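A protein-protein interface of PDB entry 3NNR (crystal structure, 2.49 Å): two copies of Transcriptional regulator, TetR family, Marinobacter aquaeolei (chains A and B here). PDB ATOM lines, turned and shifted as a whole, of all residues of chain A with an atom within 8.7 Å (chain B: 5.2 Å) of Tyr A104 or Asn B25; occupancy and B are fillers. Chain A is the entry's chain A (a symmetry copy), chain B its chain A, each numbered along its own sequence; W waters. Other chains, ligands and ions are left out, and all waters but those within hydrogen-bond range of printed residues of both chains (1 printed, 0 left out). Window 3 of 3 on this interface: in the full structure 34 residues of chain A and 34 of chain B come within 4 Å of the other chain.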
ATOM      1  N   GLU A  23     -31.258  -0.817  -1.071  1.00  0.00           N
ATOM      2  CA  GLU A  23     -31.206   0.445  -1.828  1.00  0.00           C
ATOM      3  C   GLU A  23     -32.069   0.394  -3.108  1.00  0.00           C
ATOM      4  O   GLU A  23     -32.599   1.403  -3.523  1.00  0.00           O
ATOM      5  CB  GLU A  23     -29.769   0.913  -2.118  1.00  0.00           C
ATOM      6  CG  GLU A  23     -29.159   0.442  -3.427  1.00  0.00           C
ATOM      7  CD  GLU A  23     -29.606   1.225  -4.641  1.00  0.00           C
ATOM      8  OE1 GLU A  23     -29.973   2.428  -4.552  1.00  0.00           O
ATOM      9  OE2 GLU A  23     -29.563   0.616  -5.712  1.00  0.00           O
ATOM     10  N   ARG A  24     -32.135  -0.771  -3.728  1.00  0.00           N
ATOM     11  CA  ARG A  24     -32.980  -1.071  -4.888  1.00  0.00           C
ATOM     12  C   ARG A  24     -34.378  -0.450  -4.699  1.00  0.00           C
ATOM     13  O   ARG A  24     -34.884   0.255  -5.570  1.00  0.00           O
ATOM     14  CB  ARG A  24     -33.187  -2.592  -4.977  1.00  0.00           C
ATOM     15  CG  ARG A  24     -32.939  -3.259  -6.311  1.00  0.00           C
ATOM     16  CD  ARG A  24     -33.871  -4.440  -6.564  1.00  0.00           C
ATOM     17  NE  ARG A  24     -33.179  -5.671  -6.933  1.00  0.00           N
ATOM     18  CZ  ARG A  24     -33.742  -6.735  -7.547  1.00  0.00           C
ATOM     19  NH1 ARG A  24     -35.028  -6.763  -7.973  1.00  0.00           N
ATOM     20  NH2 ARG A  24     -32.972  -7.797  -7.785  1.00  0.00           N
ATOM     21  N   SER A  50     -27.673   8.828  -5.932  1.00  0.00           N
ATOM     22  CA  SER A  50     -26.228   8.487  -6.072  1.00  0.00           C
ATOM     23  C   SER A  50     -25.316   9.347  -5.219  1.00  0.00           C
ATOM     24  O   SER A  50     -24.261   8.884  -4.775  1.00  0.00           O
ATOM     25  CB  SER A  50     -25.748   8.618  -7.524  1.00  0.00           C
ATOM     26  OG  SER A  50     -26.440   7.717  -8.356  1.00  0.00           O
ATOM     27  N   ILE A  53     -25.564   8.053  -1.669  1.00  0.00           N
ATOM     28  CA  ILE A  53     -24.774   6.825  -1.563  1.00  0.00           C
ATOM     29  C   ILE A  53     -23.264   7.108  -1.530  1.00  0.00           C
ATOM     30  O   ILE A  53     -22.545   6.521  -0.703  1.00  0.00           O
ATOM     31  CB  ILE A  53     -25.119   5.853  -2.697  1.00  0.00           C
ATOM     32  CG1 ILE A  53     -26.562   5.347  -2.552  1.00  0.00           C
ATOM     33  CG2 ILE A  53     -24.162   4.629  -2.698  1.00  0.00           C
ATOM     34  CD1 ILE A  53     -27.056   4.602  -3.794  1.00  0.00           C
ATOM     35  N   PHE A  98     -24.340  -1.712   1.130  1.00  0.00           N
ATOM     36  CA  PHE A  98     -23.332  -1.451   0.108  1.00  0.00           C
ATOM     37  C   PHE A  98     -22.888  -2.713  -0.634  1.00  0.00           C
ATOM     38  O   PHE A  98     -23.063  -2.808  -1.849  1.00  0.00           O
ATOM     39  CB  PHE A  98     -22.161  -0.712   0.737  1.00  0.00           C
ATOM     40  CG  PHE A  98     -21.175  -0.200  -0.240  1.00  0.00           C
ATOM     41  CD1 PHE A  98     -21.430   0.959  -0.940  1.00  0.00           C
ATOM     42  CD2 PHE A  98     -19.964  -0.846  -0.430  1.00  0.00           C
ATOM     43  CE1 PHE A  98     -20.514   1.447  -1.849  1.00  0.00           C
ATOM     44  CE2 PHE A  98     -19.041  -0.366  -1.331  1.00  0.00           C
ATOM     45  CZ  PHE A  98     -19.320   0.779  -2.049  1.00  0.00           C
ATOM     46  N   HIS A  99     -22.393  -3.702   0.101  1.00  0.00           N
ATOM     47  CA  HIS A  99     -21.918  -4.958  -0.533  1.00  0.00           C
ATOM     48  C   HIS A  99     -23.017  -5.792  -1.187  1.00  0.00           C
ATOM     49  O   HIS A  99     -22.738  -6.582  -2.098  1.00  0.00           O
ATOM     50  CB  HIS A  99     -21.094  -5.783   0.439  1.00  0.00           C
ATOM     51  CG  HIS A  99     -19.926  -5.024   0.972  1.00  0.00           C
ATOM     52  ND1 HIS A  99     -20.035  -4.171   2.052  1.00  0.00           N
ATOM     53  CD2 HIS A  99     -18.645  -4.931   0.535  1.00  0.00           C
ATOM     54  CE1 HIS A  99     -18.858  -3.610   2.272  1.00  0.00           C
ATOM     55  NE2 HIS A  99     -17.996  -4.056   1.371  1.00  0.00           N
ATOM     56  N   ARG A 100     -24.253  -5.563  -0.758  1.00  0.00           N
ATOM     57  CA  ARG A 100     -25.414  -6.271  -1.266  1.00  0.00           C
ATOM     58  C   ARG A 100     -25.744  -5.868  -2.706  1.00  0.00           C
ATOM     59  O   ARG A 100     -26.034  -6.738  -3.529  1.00  0.00           O
ATOM     60  CB  ARG A 100     -26.581  -6.018  -0.335  1.00  0.00           C
ATOM     61  CG  ARG A 100     -27.877  -6.706  -0.694  1.00  0.00           C
ATOM     62  CD  ARG A 100     -28.752  -6.749   0.552  1.00  0.00           C
ATOM     63  NE  ARG A 100     -29.165  -5.436   0.984  1.00  0.00           N
ATOM     64  CZ  ARG A 100     -29.537  -5.081   2.216  1.00  0.00           C
ATOM     65  NH1 ARG A 100     -29.495  -5.902   3.246  1.00  0.00           N
ATOM     66  NH2 ARG A 100     -29.924  -3.834   2.422  1.00  0.00           N
ATOM     67  N   ASP A 101     -25.680  -4.567  -2.999  1.00  0.00           N
ATOM     68  CA  ASP A 101     -25.968  -4.034  -4.318  1.00  0.00           C
ATOM     69  C   ASP A 101     -24.700  -3.490  -4.965  1.00  0.00           C
ATOM     70  O   ASP A 101     -24.762  -2.676  -5.909  1.00  0.00           O
ATOM     71  CB  ASP A 101     -27.096  -2.980  -4.225  1.00  0.00           C
ATOM     72  CG  ASP A 101     -28.488  -3.600  -4.250  1.00  0.00           C
ATOM     73  OD1 ASP A 101     -28.706  -4.542  -5.049  1.00  0.00           O
ATOM     74  OD2 ASP A 101     -29.395  -3.086  -3.558  1.00  0.00           O
ATOM     75  N   LEU A 102     -23.560  -4.056  -4.578  1.00  0.00           N
ATOM     76  CA  LEU A 102     -22.270  -3.477  -4.968  1.00  0.00           C
ATOM     77  C   LEU A 102     -22.153  -3.185  -6.450  1.00  0.00           C
ATOM     78  O   LEU A 102     -21.909  -2.059  -6.838  1.00  0.00           O
ATOM     79  CB  LEU A 102     -21.101  -4.383  -4.519  1.00  0.00           C
ATOM     80  CG  LEU A 102     -19.654  -3.873  -4.683  1.00  0.00           C
ATOM     81  CD1 LEU A 102     -19.524  -2.523  -4.017  1.00  0.00           C
ATOM     82  CD2 LEU A 102     -18.597  -4.890  -4.153  1.00  0.00           C
ATOM     83  N   GLU A 103     -22.441  -4.187  -7.268  1.00  0.00           N
ATOM     84  CA  GLU A 103     -22.203  -4.087  -8.689  1.00  0.00           C
ATOM     85  C   GLU A 103     -23.071  -3.048  -9.387  1.00  0.00           C
ATOM     86  O   GLU A 103     -22.596  -2.363 -10.309  1.00  0.00           O
ATOM     87  CB  GLU A 103     -22.243  -5.480  -9.284  1.00  0.00           C
ATOM     88  CG  GLU A 103     -21.889  -5.566 -10.757  1.00  0.00           C
ATOM     89  CD  GLU A 103     -21.686  -6.983 -11.238  1.00  0.00           C
ATOM     90  OE1 GLU A 103     -21.549  -7.920 -10.390  1.00  0.00           O
ATOM     91  OE2 GLU A 103     -21.661  -7.149 -12.479  1.00  0.00           O
ATOM     92  N   TYR A 104     -24.304  -2.861  -8.932  1.00  0.00           N
ATOM     93  CA  TYR A 104     -25.138  -1.786  -9.510  1.00  0.00           C
ATOM     94  C   TYR A 104     -24.647  -0.407  -9.068  1.00  0.00           C
ATOM     95  O   TYR A 104     -24.719   0.566  -9.821  1.00  0.00           O
ATOM     96  CB  TYR A 104     -26.604  -1.951  -9.132  1.00  0.00           C
ATOM     97  CG  TYR A 104     -27.216  -3.187  -9.705  1.00  0.00           C
ATOM     98  CD1 TYR A 104     -27.744  -3.191 -11.000  1.00  0.00           C
ATOM     99  CD2 TYR A 104     -27.242  -4.382  -8.980  1.00  0.00           C
ATOM    100  CE1 TYR A 104     -28.319  -4.359 -11.546  1.00  0.00           C
ATOM    101  CE2 TYR A 104     -27.799  -5.548  -9.524  1.00  0.00           C
ATOM    102  CZ  TYR A 104     -28.348  -5.526 -10.799  1.00  0.00           C
ATOM    103  OH  TYR A 104     -28.926  -6.631 -11.341  1.00  0.00           O
ATOM    104  N   LEU A 105     -24.167  -0.322  -7.830  1.00  0.00           N
ATOM    105  CA  LEU A 105     -23.673   0.948  -7.284  1.00  0.00           C
ATOM    106  C   LEU A 105     -22.391   1.402  -8.036  1.00  0.00           C
ATOM    107  O   LEU A 105     -22.312   2.542  -8.481  1.00  0.00           O
ATOM    108  CB  LEU A 105     -23.527   0.841  -5.770  1.00  0.00           C
ATOM    109  CG  LEU A 105     -24.890   0.658  -5.053  1.00  0.00           C
ATOM    110  CD1 LEU A 105     -24.709   0.406  -3.566  1.00  0.00           C
ATOM    111  CD2 LEU A 105     -25.818   1.862  -5.262  1.00  0.00           C
ATOM    112  N   LEU A 106     -21.458   0.485  -8.281  1.00  0.00           N
ATOM    113  CA  LEU A 106     -20.279   0.815  -9.086  1.00  0.00           C
ATOM    114  C   LEU A 106     -20.656   1.254 -10.518  1.00  0.00           C
ATOM    115  O   LEU A 106     -20.157   2.261 -11.015  1.00  0.00           O
ATOM    116  CB  LEU A 106     -19.279  -0.341  -9.102  1.00  0.00           C
ATOM    117  CG  LEU A 106     -18.792  -0.851  -7.728  1.00  0.00           C
ATOM    118  CD1 LEU A 106     -17.521  -1.687  -7.880  1.00  0.00           C
ATOM    119  CD2 LEU A 106     -18.567   0.257  -6.728  1.00  0.00           C
ATOM    120  N   ASP A 107     -21.566   0.527 -11.147  1.00  0.00           N
ATOM    121  CA  ASP A 107     -22.047   0.866 -12.487  1.00  0.00           C
ATOM    122  C   ASP A 107     -22.805   2.208 -12.522  1.00  0.00           C
ATOM    123  O   ASP A 107     -22.743   2.927 -13.520  1.00  0.00           O
ATOM    124  CB  ASP A 107     -22.946  -0.269 -13.011  1.00  0.00           C
ATOM    125  CG  ASP A 107     -23.498   0.003 -14.371  1.00  0.00           C
ATOM    126  OD1 ASP A 107     -22.770  -0.215 -15.354  1.00  0.00           O
ATOM    127  OD2 ASP A 107     -24.673   0.416 -14.444  1.00  0.00           O
ATOM    128  N   SER A 108     -23.534   2.534 -11.459  1.00  0.00           N
ATOM    129  CA  SER A 108     -24.252   3.818 -11.408  1.00  0.00           C
ATOM    130  C   SER A 108     -23.339   5.046 -11.282  1.00  0.00           C
ATOM    131  O   SER A 108     -23.691   6.120 -11.791  1.00  0.00           O
ATOM    132  CB  SER A 108     -25.287   3.834 -10.276  1.00  0.00           C
ATOM    133  OG  SER A 108     -26.380   2.982 -10.603  1.00  0.00           O
ATOM    134  N   ASP A 109     -22.162   4.868 -10.669  1.00  0.00           N
ATOM    135  CA  ASP A 109     -21.305   5.976 -10.328  1.00  0.00           C
ATOM    136  C   ASP A 109     -19.813   5.728 -10.560  1.00  0.00           C
ATOM    137  O   ASP A 109     -19.154   5.001  -9.796  1.00  0.00           O
ATOM    138  CB  ASP A 109     -21.574   6.334  -8.864  1.00  0.00           C
ATOM    139  CG  ASP A 109     -21.024   7.694  -8.473  1.00  0.00           C
ATOM    140  OD1 ASP A 109     -20.181   8.257  -9.196  1.00  0.00           O
ATOM    141  OD2 ASP A 109     -21.452   8.220  -7.418  1.00  0.00           O
ATOM    142  N   PRO A 110     -19.260   6.378 -11.594  1.00  0.00           N
ATOM    143  CA  PRO A 110     -17.815   6.270 -11.851  1.00  0.00           C
ATOM    144  C   PRO A 110     -16.908   6.761 -10.735  1.00  0.00           C
ATOM    145  O   PRO A 110     -15.794   6.262 -10.612  1.00  0.00           O
ATOM    146  CB  PRO A 110     -17.630   7.116 -13.102  1.00  0.00           C
ATOM    147  CG  PRO A 110     -18.899   6.884 -13.854  1.00  0.00           C
ATOM    148  CD  PRO A 110     -19.980   6.822 -12.799  1.00  0.00           C
ATOM    149  N   LEU A 112     -17.622   6.497  -7.498  1.00  0.00           N
ATOM    150  CA  LEU A 112     -17.694   5.414  -6.515  1.00  0.00           C
ATOM    151  C   LEU A 112     -16.857   4.225  -6.948  1.00  0.00           C
ATOM    152  O   LEU A 112     -16.132   3.653  -6.165  1.00  0.00           O
ATOM    153  CB  LEU A 112     -19.145   5.006  -6.328  1.00  0.00           C
ATOM    154  CG  LEU A 112     -19.510   4.073  -5.185  1.00  0.00           C
ATOM    155  CD1 LEU A 112     -19.008   4.624  -3.914  1.00  0.00           C
ATOM    156  CD2 LEU A 112     -21.037   3.912  -5.126  1.00  0.00           C
ATOM    157  N   ARG A 113     -16.944   3.882  -8.219  1.00  0.00           N
ATOM    158  CA  ARG A 113     -16.162   2.795  -8.814  1.00  0.00           C
ATOM    159  C   ARG A 113     -14.668   3.071  -8.666  1.00  0.00           C
ATOM    160  O   ARG A 113     -13.915   2.206  -8.223  1.00  0.00           O
ATOM    161  CB  ARG A 113     -16.514   2.675 -10.309  1.00  0.00           C
ATOM    162  CG  ARG A 113     -15.921   1.499 -11.092  1.00  0.00           C
ATOM    163  CD  ARG A 113     -16.104   1.778 -12.613  1.00  0.00           C
ATOM    164  NE  ARG A 113     -17.498   2.130 -12.958  1.00  0.00           N
ATOM    165  CZ  ARG A 113     -17.905   2.890 -13.996  1.00  0.00           C
ATOM    166  NH1 ARG A 113     -17.040   3.457 -14.871  1.00  0.00           N
ATOM    167  NH2 ARG A 113     -19.218   3.115 -14.154  1.00  0.00           N
ATOM    168  N   LYS B  21     -27.939  -7.135 -18.710  1.00  0.00           N
ATOM    169  CA  LYS B  21     -28.501  -5.876 -18.139  1.00  0.00           C
ATOM    170  C   LYS B  21     -28.762  -5.888 -16.616  1.00  0.00           C
ATOM    171  O   LYS B  21     -28.934  -4.834 -16.032  1.00  0.00           O
ATOM    172  CB  LYS B  21     -29.823  -5.510 -18.838  1.00  0.00           C
ATOM    173  CG  LYS B  21     -29.822  -5.385 -20.364  1.00  0.00           C
ATOM    174  CD  LYS B  21     -29.049  -4.231 -20.872  1.00  0.00           C
ATOM    175  CE  LYS B  21     -29.251  -4.071 -22.391  1.00  0.00           C
ATOM    176  NZ  LYS B  21     -28.266  -3.111 -23.011  1.00  0.00           N
ATOM    177  N   GLY B  22     -28.811  -7.056 -15.987  1.00  0.00           N
ATOM    178  CA  GLY B  22     -29.112  -7.176 -14.552  1.00  0.00           C
ATOM    179  C   GLY B  22     -30.574  -7.545 -14.419  1.00  0.00           C
ATOM    180  O   GLY B  22     -31.418  -6.914 -15.065  1.00  0.00           O
ATOM    181  N   GLU B  23     -30.903  -8.526 -13.583  1.00  0.00           N
ATOM    182  CA  GLU B  23     -32.322  -8.884 -13.422  1.00  0.00           C
ATOM    183  C   GLU B  23     -33.164  -7.706 -12.884  1.00  0.00           C
ATOM    184  O   GLU B  23     -34.329  -7.595 -13.207  1.00  0.00           O
ATOM    185  CB  GLU B  23     -32.528 -10.166 -12.595  1.00  0.00           C
ATOM    186  CG  GLU B  23     -32.706  -9.980 -11.098  1.00  0.00           C
ATOM    187  CD  GLU B  23     -34.095  -9.550 -10.684  1.00  0.00           C
ATOM    188  OE1 GLU B  23     -35.109  -9.840 -11.374  1.00  0.00           O
ATOM    189  OE2 GLU B  23     -34.164  -8.924  -9.624  1.00  0.00           O
ATOM    190  N   ARG B  24     -32.565  -6.894 -12.031  1.00  0.00           N
ATOM    191  CA  ARG B  24     -33.137  -5.658 -11.488  1.00  0.00           C
ATOM    192  C   ARG B  24     -33.861  -4.876 -12.602  1.00  0.00           C
ATOM    193  O   ARG B  24     -35.017  -4.483 -12.455  1.00  0.00           O
ATOM    194  CB  ARG B  24     -31.996  -4.754 -10.993  1.00  0.00           C
ATOM    195  CG  ARG B  24     -32.111  -4.174  -9.601  1.00  0.00           C
ATOM    196  CD  ARG B  24     -31.501  -2.781  -9.489  1.00  0.00           C
ATOM    197  NE  ARG B  24     -30.539  -2.642  -8.399  1.00  0.00           N
ATOM    198  CZ  ARG B  24     -30.133  -1.474  -7.854  1.00  0.00           C
ATOM    199  NH1 ARG B  24     -30.633  -0.266  -8.206  1.00  0.00           N
ATOM    200  NH2 ARG B  24     -29.220  -1.524  -6.883  1.00  0.00           N
ATOM    201  N   ASN B  25     -33.174  -4.721 -13.736  1.00  0.00           N
ATOM    202  CA  ASN B  25     -33.625  -3.889 -14.851  1.00  0.00           C
ATOM    203  C   ASN B  25     -34.395  -4.597 -15.950  1.00  0.00           C
ATOM    204  O   ASN B  25     -34.709  -3.973 -16.945  1.00  0.00           O
ATOM    205  CB  ASN B  25     -32.425  -3.210 -15.517  1.00  0.00           C
ATOM    206  CG  ASN B  25     -31.575  -2.426 -14.556  1.00  0.00           C
ATOM    207  OD1 ASN B  25     -30.387  -2.676 -14.468  1.00  0.00           O
ATOM    208  ND2 ASN B  25     -32.176  -1.485 -13.819  1.00  0.00           N
ATOM    209  N   ILE B  26     -34.689  -5.877 -15.799  1.00  0.00           N
ATOM    210  CA  ILE B  26     -35.419  -6.607 -16.836  1.00  0.00           C
ATOM    211  C   ILE B  26     -36.777  -7.032 -16.305  1.00  0.00           C
ATOM    212  O   ILE B  26     -36.866  -7.632 -15.243  1.00  0.00           O
ATOM    213  CB  ILE B  26     -34.598  -7.800 -17.365  1.00  0.00           C
ATOM    214  CG1 ILE B  26     -33.269  -7.306 -18.000  1.00  0.00           C
ATOM    215  CG2 ILE B  26     -35.413  -8.630 -18.341  1.00  0.00           C
ATOM    216  CD1 ILE B  26     -33.392  -6.341 -19.183  1.00  0.00           C
ATOM    217  N   THR B  27     -37.815  -6.691 -17.065  1.00  0.00           N
ATOM    218  CA  THR B  27     -39.223  -7.041 -16.787  1.00  0.00           C
ATOM    219  C   THR B  27     -39.716  -8.050 -17.827  1.00  0.00           C
ATOM    220  O   THR B  27     -39.097  -8.254 -18.886  1.00  0.00           O
ATOM    221  CB  THR B  27     -40.140  -5.783 -16.882  1.00  0.00           C
ATOM    222  OG1 THR B  27     -40.162  -5.283 -18.231  1.00  0.00           O
ATOM    223  CG2 THR B  27     -39.616  -4.675 -15.949  1.00  0.00           C
ATOM    224  N   HIS B  30     -40.027  -6.561 -21.298  1.00  0.00           N
ATOM    225  CA  HIS B  30     -38.755  -6.503 -22.036  1.00  0.00           C
ATOM    226  C   HIS B  30     -38.486  -7.849 -22.694  1.00  0.00           C
ATOM    227  O   HIS B  30     -38.100  -7.893 -23.866  1.00  0.00           O
ATOM    228  CB  HIS B  30     -37.528  -6.190 -21.153  1.00  0.00           C
ATOM    229  CG  HIS B  30     -37.486  -4.805 -20.584  1.00  0.00           C
ATOM    230  ND1 HIS B  30     -37.841  -4.521 -19.285  1.00  0.00           N
ATOM    231  CD2 HIS B  30     -37.056  -3.635 -21.113  1.00  0.00           C
ATOM    232  CE1 HIS B  30     -37.671  -3.233 -19.049  1.00  0.00           C
ATOM    233  NE2 HIS B  30     -37.199  -2.671 -20.143  1.00  0.00           N
ATOM    234  N   ARG B 100     -25.269 -12.131  -8.393  1.00  0.00           N
ATOM    235  CA  ARG B 100     -25.232 -10.680  -8.374  1.00  0.00           C
ATOM    236  C   ARG B 100     -26.407 -10.089  -7.589  1.00  0.00           C
ATOM    237  O   ARG B 100     -26.207  -9.159  -6.806  1.00  0.00           O
ATOM    238  CB  ARG B 100     -25.207 -10.178  -9.803  1.00  0.00           C
ATOM    239  CG  ARG B 100     -25.139  -8.679  -9.978  1.00  0.00           C
ATOM    240  CD  ARG B 100     -24.637  -8.389 -11.387  1.00  0.00           C
ATOM    241  NE  ARG B 100     -25.568  -8.815 -12.404  1.00  0.00           N
ATOM    242  CZ  ARG B 100     -25.282  -9.112 -13.673  1.00  0.00           C
ATOM    243  NH1 ARG B 100     -24.053  -9.131 -14.150  1.00  0.00           N
ATOM    244  NH2 ARG B 100     -26.274  -9.449 -14.479  1.00  0.00           N
ATOM    245  N   ASP B 101     -27.606 -10.640  -7.791  1.00  0.00           N
ATOM    246  CA  ASP B 101     -28.812 -10.186  -7.122  1.00  0.00           C
ATOM    247  C   ASP B 101     -29.309 -11.239  -6.139  1.00  0.00           C
ATOM    248  O   ASP B 101     -30.490 -11.231  -5.737  1.00  0.00           O
ATOM    249  CB  ASP B 101     -29.878  -9.790  -8.170  1.00  0.00           C
ATOM    250  CG  ASP B 101     -29.708  -8.362  -8.677  1.00  0.00           C
ATOM    251  OD1 ASP B 101     -29.420  -7.466  -7.848  1.00  0.00           O
ATOM    252  OD2 ASP B 101     -29.963  -8.108  -9.875  1.00  0.00           O
HETATM  253  O   HOH W   1     -28.803  -9.938 -11.727  1.00  0.00           O
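OE2 of Glu B23 is in salt-bridge range of NH2 of Arg A24, 2.5 Å away. The guanidinium group (NH2) of Arg B24 lies within salt-bridge range of the side-chain carboxylate (OE2) of Glu A23 (2.5 Å). The side-chain carboxylate (OD1) of Asp A101 is in salt-bridge range of the guanidinium group (NH2) of Arg B24. NH1 of Arg B100 lies within salt-bridge range of OE2 of Glu A103 (3.5 Å). OD1 of Asp B101 lies within salt-bridge range of NH2 of Arg A24. The side-chain hydroxyl of Tyr A104 sits close to the side-chain carboxylate of Asp B101 (2.3 Å).
The side-chain amide oxygen (OD1) of Asn B25 sits close to the backbone carbonyl oxygen (O) of Lys B21, 3.0 Å away. The backbone carbonyl oxygen of Tyr A104 sits at hydrogen-bond distance from the side-chain hydroxyl of Ser A108, at 3.0 Å.
Among the printed residues, merely in contact across the chains: Arg A24 with Arg B24, Tyr A104 with Gly B22, Tyr A104 with Glu B23, Tyr A104 with Arg B24 and Tyr A104 with Asn B25.
Tyr A104 touches five residues of chain B. Asn B25 touches one residue of chain A. Of the printed residues of chain A, Gly B22 touches Tyr A104. Of the printed residues of chain A, Glu B23 touches Arg A24 and Tyr A104. Pro A110 touches none of the printed residues of chain B. Asp A107 touches none of the printed residues of chain B. The nearest residue of chain B that does not touch Tyr A104 is Arg B100 (4.1 Å). The nearest residue of chain A that does not touch Asn B25 is Arg A24 (6.4 Å).
Hydrophobic or aromatic side chains of chain A that line the printed part of chain B: Tyr A104. Printed residues of chain B that touch a printed residue of chain A: Gly B22, Glu B23, Arg B24, Asn B25, Arg B100 and Asp B101. Among the printed residues, 11 pairs touch across the chains.
Glu A23 touches Arg B24, and with the chains exchanged Arg A24 touches Glu B23. Arg B24 touches its own counterpart, Arg A24. Arg A24 touches Asp B101, and with the chains exchanged Asp A101 touches Arg B24. Of the 11 pairs that touch across the chains among the printed residues, 5 have their exchanged pair printed and touching as well.
Water W1 lies within hydrogen-bond range of the side-chain carboxylate of Asp B101, the backbone NH of Glu B23, the side-chain hydroxyl of Tyr A104 and the guanidinium group of Arg B100.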
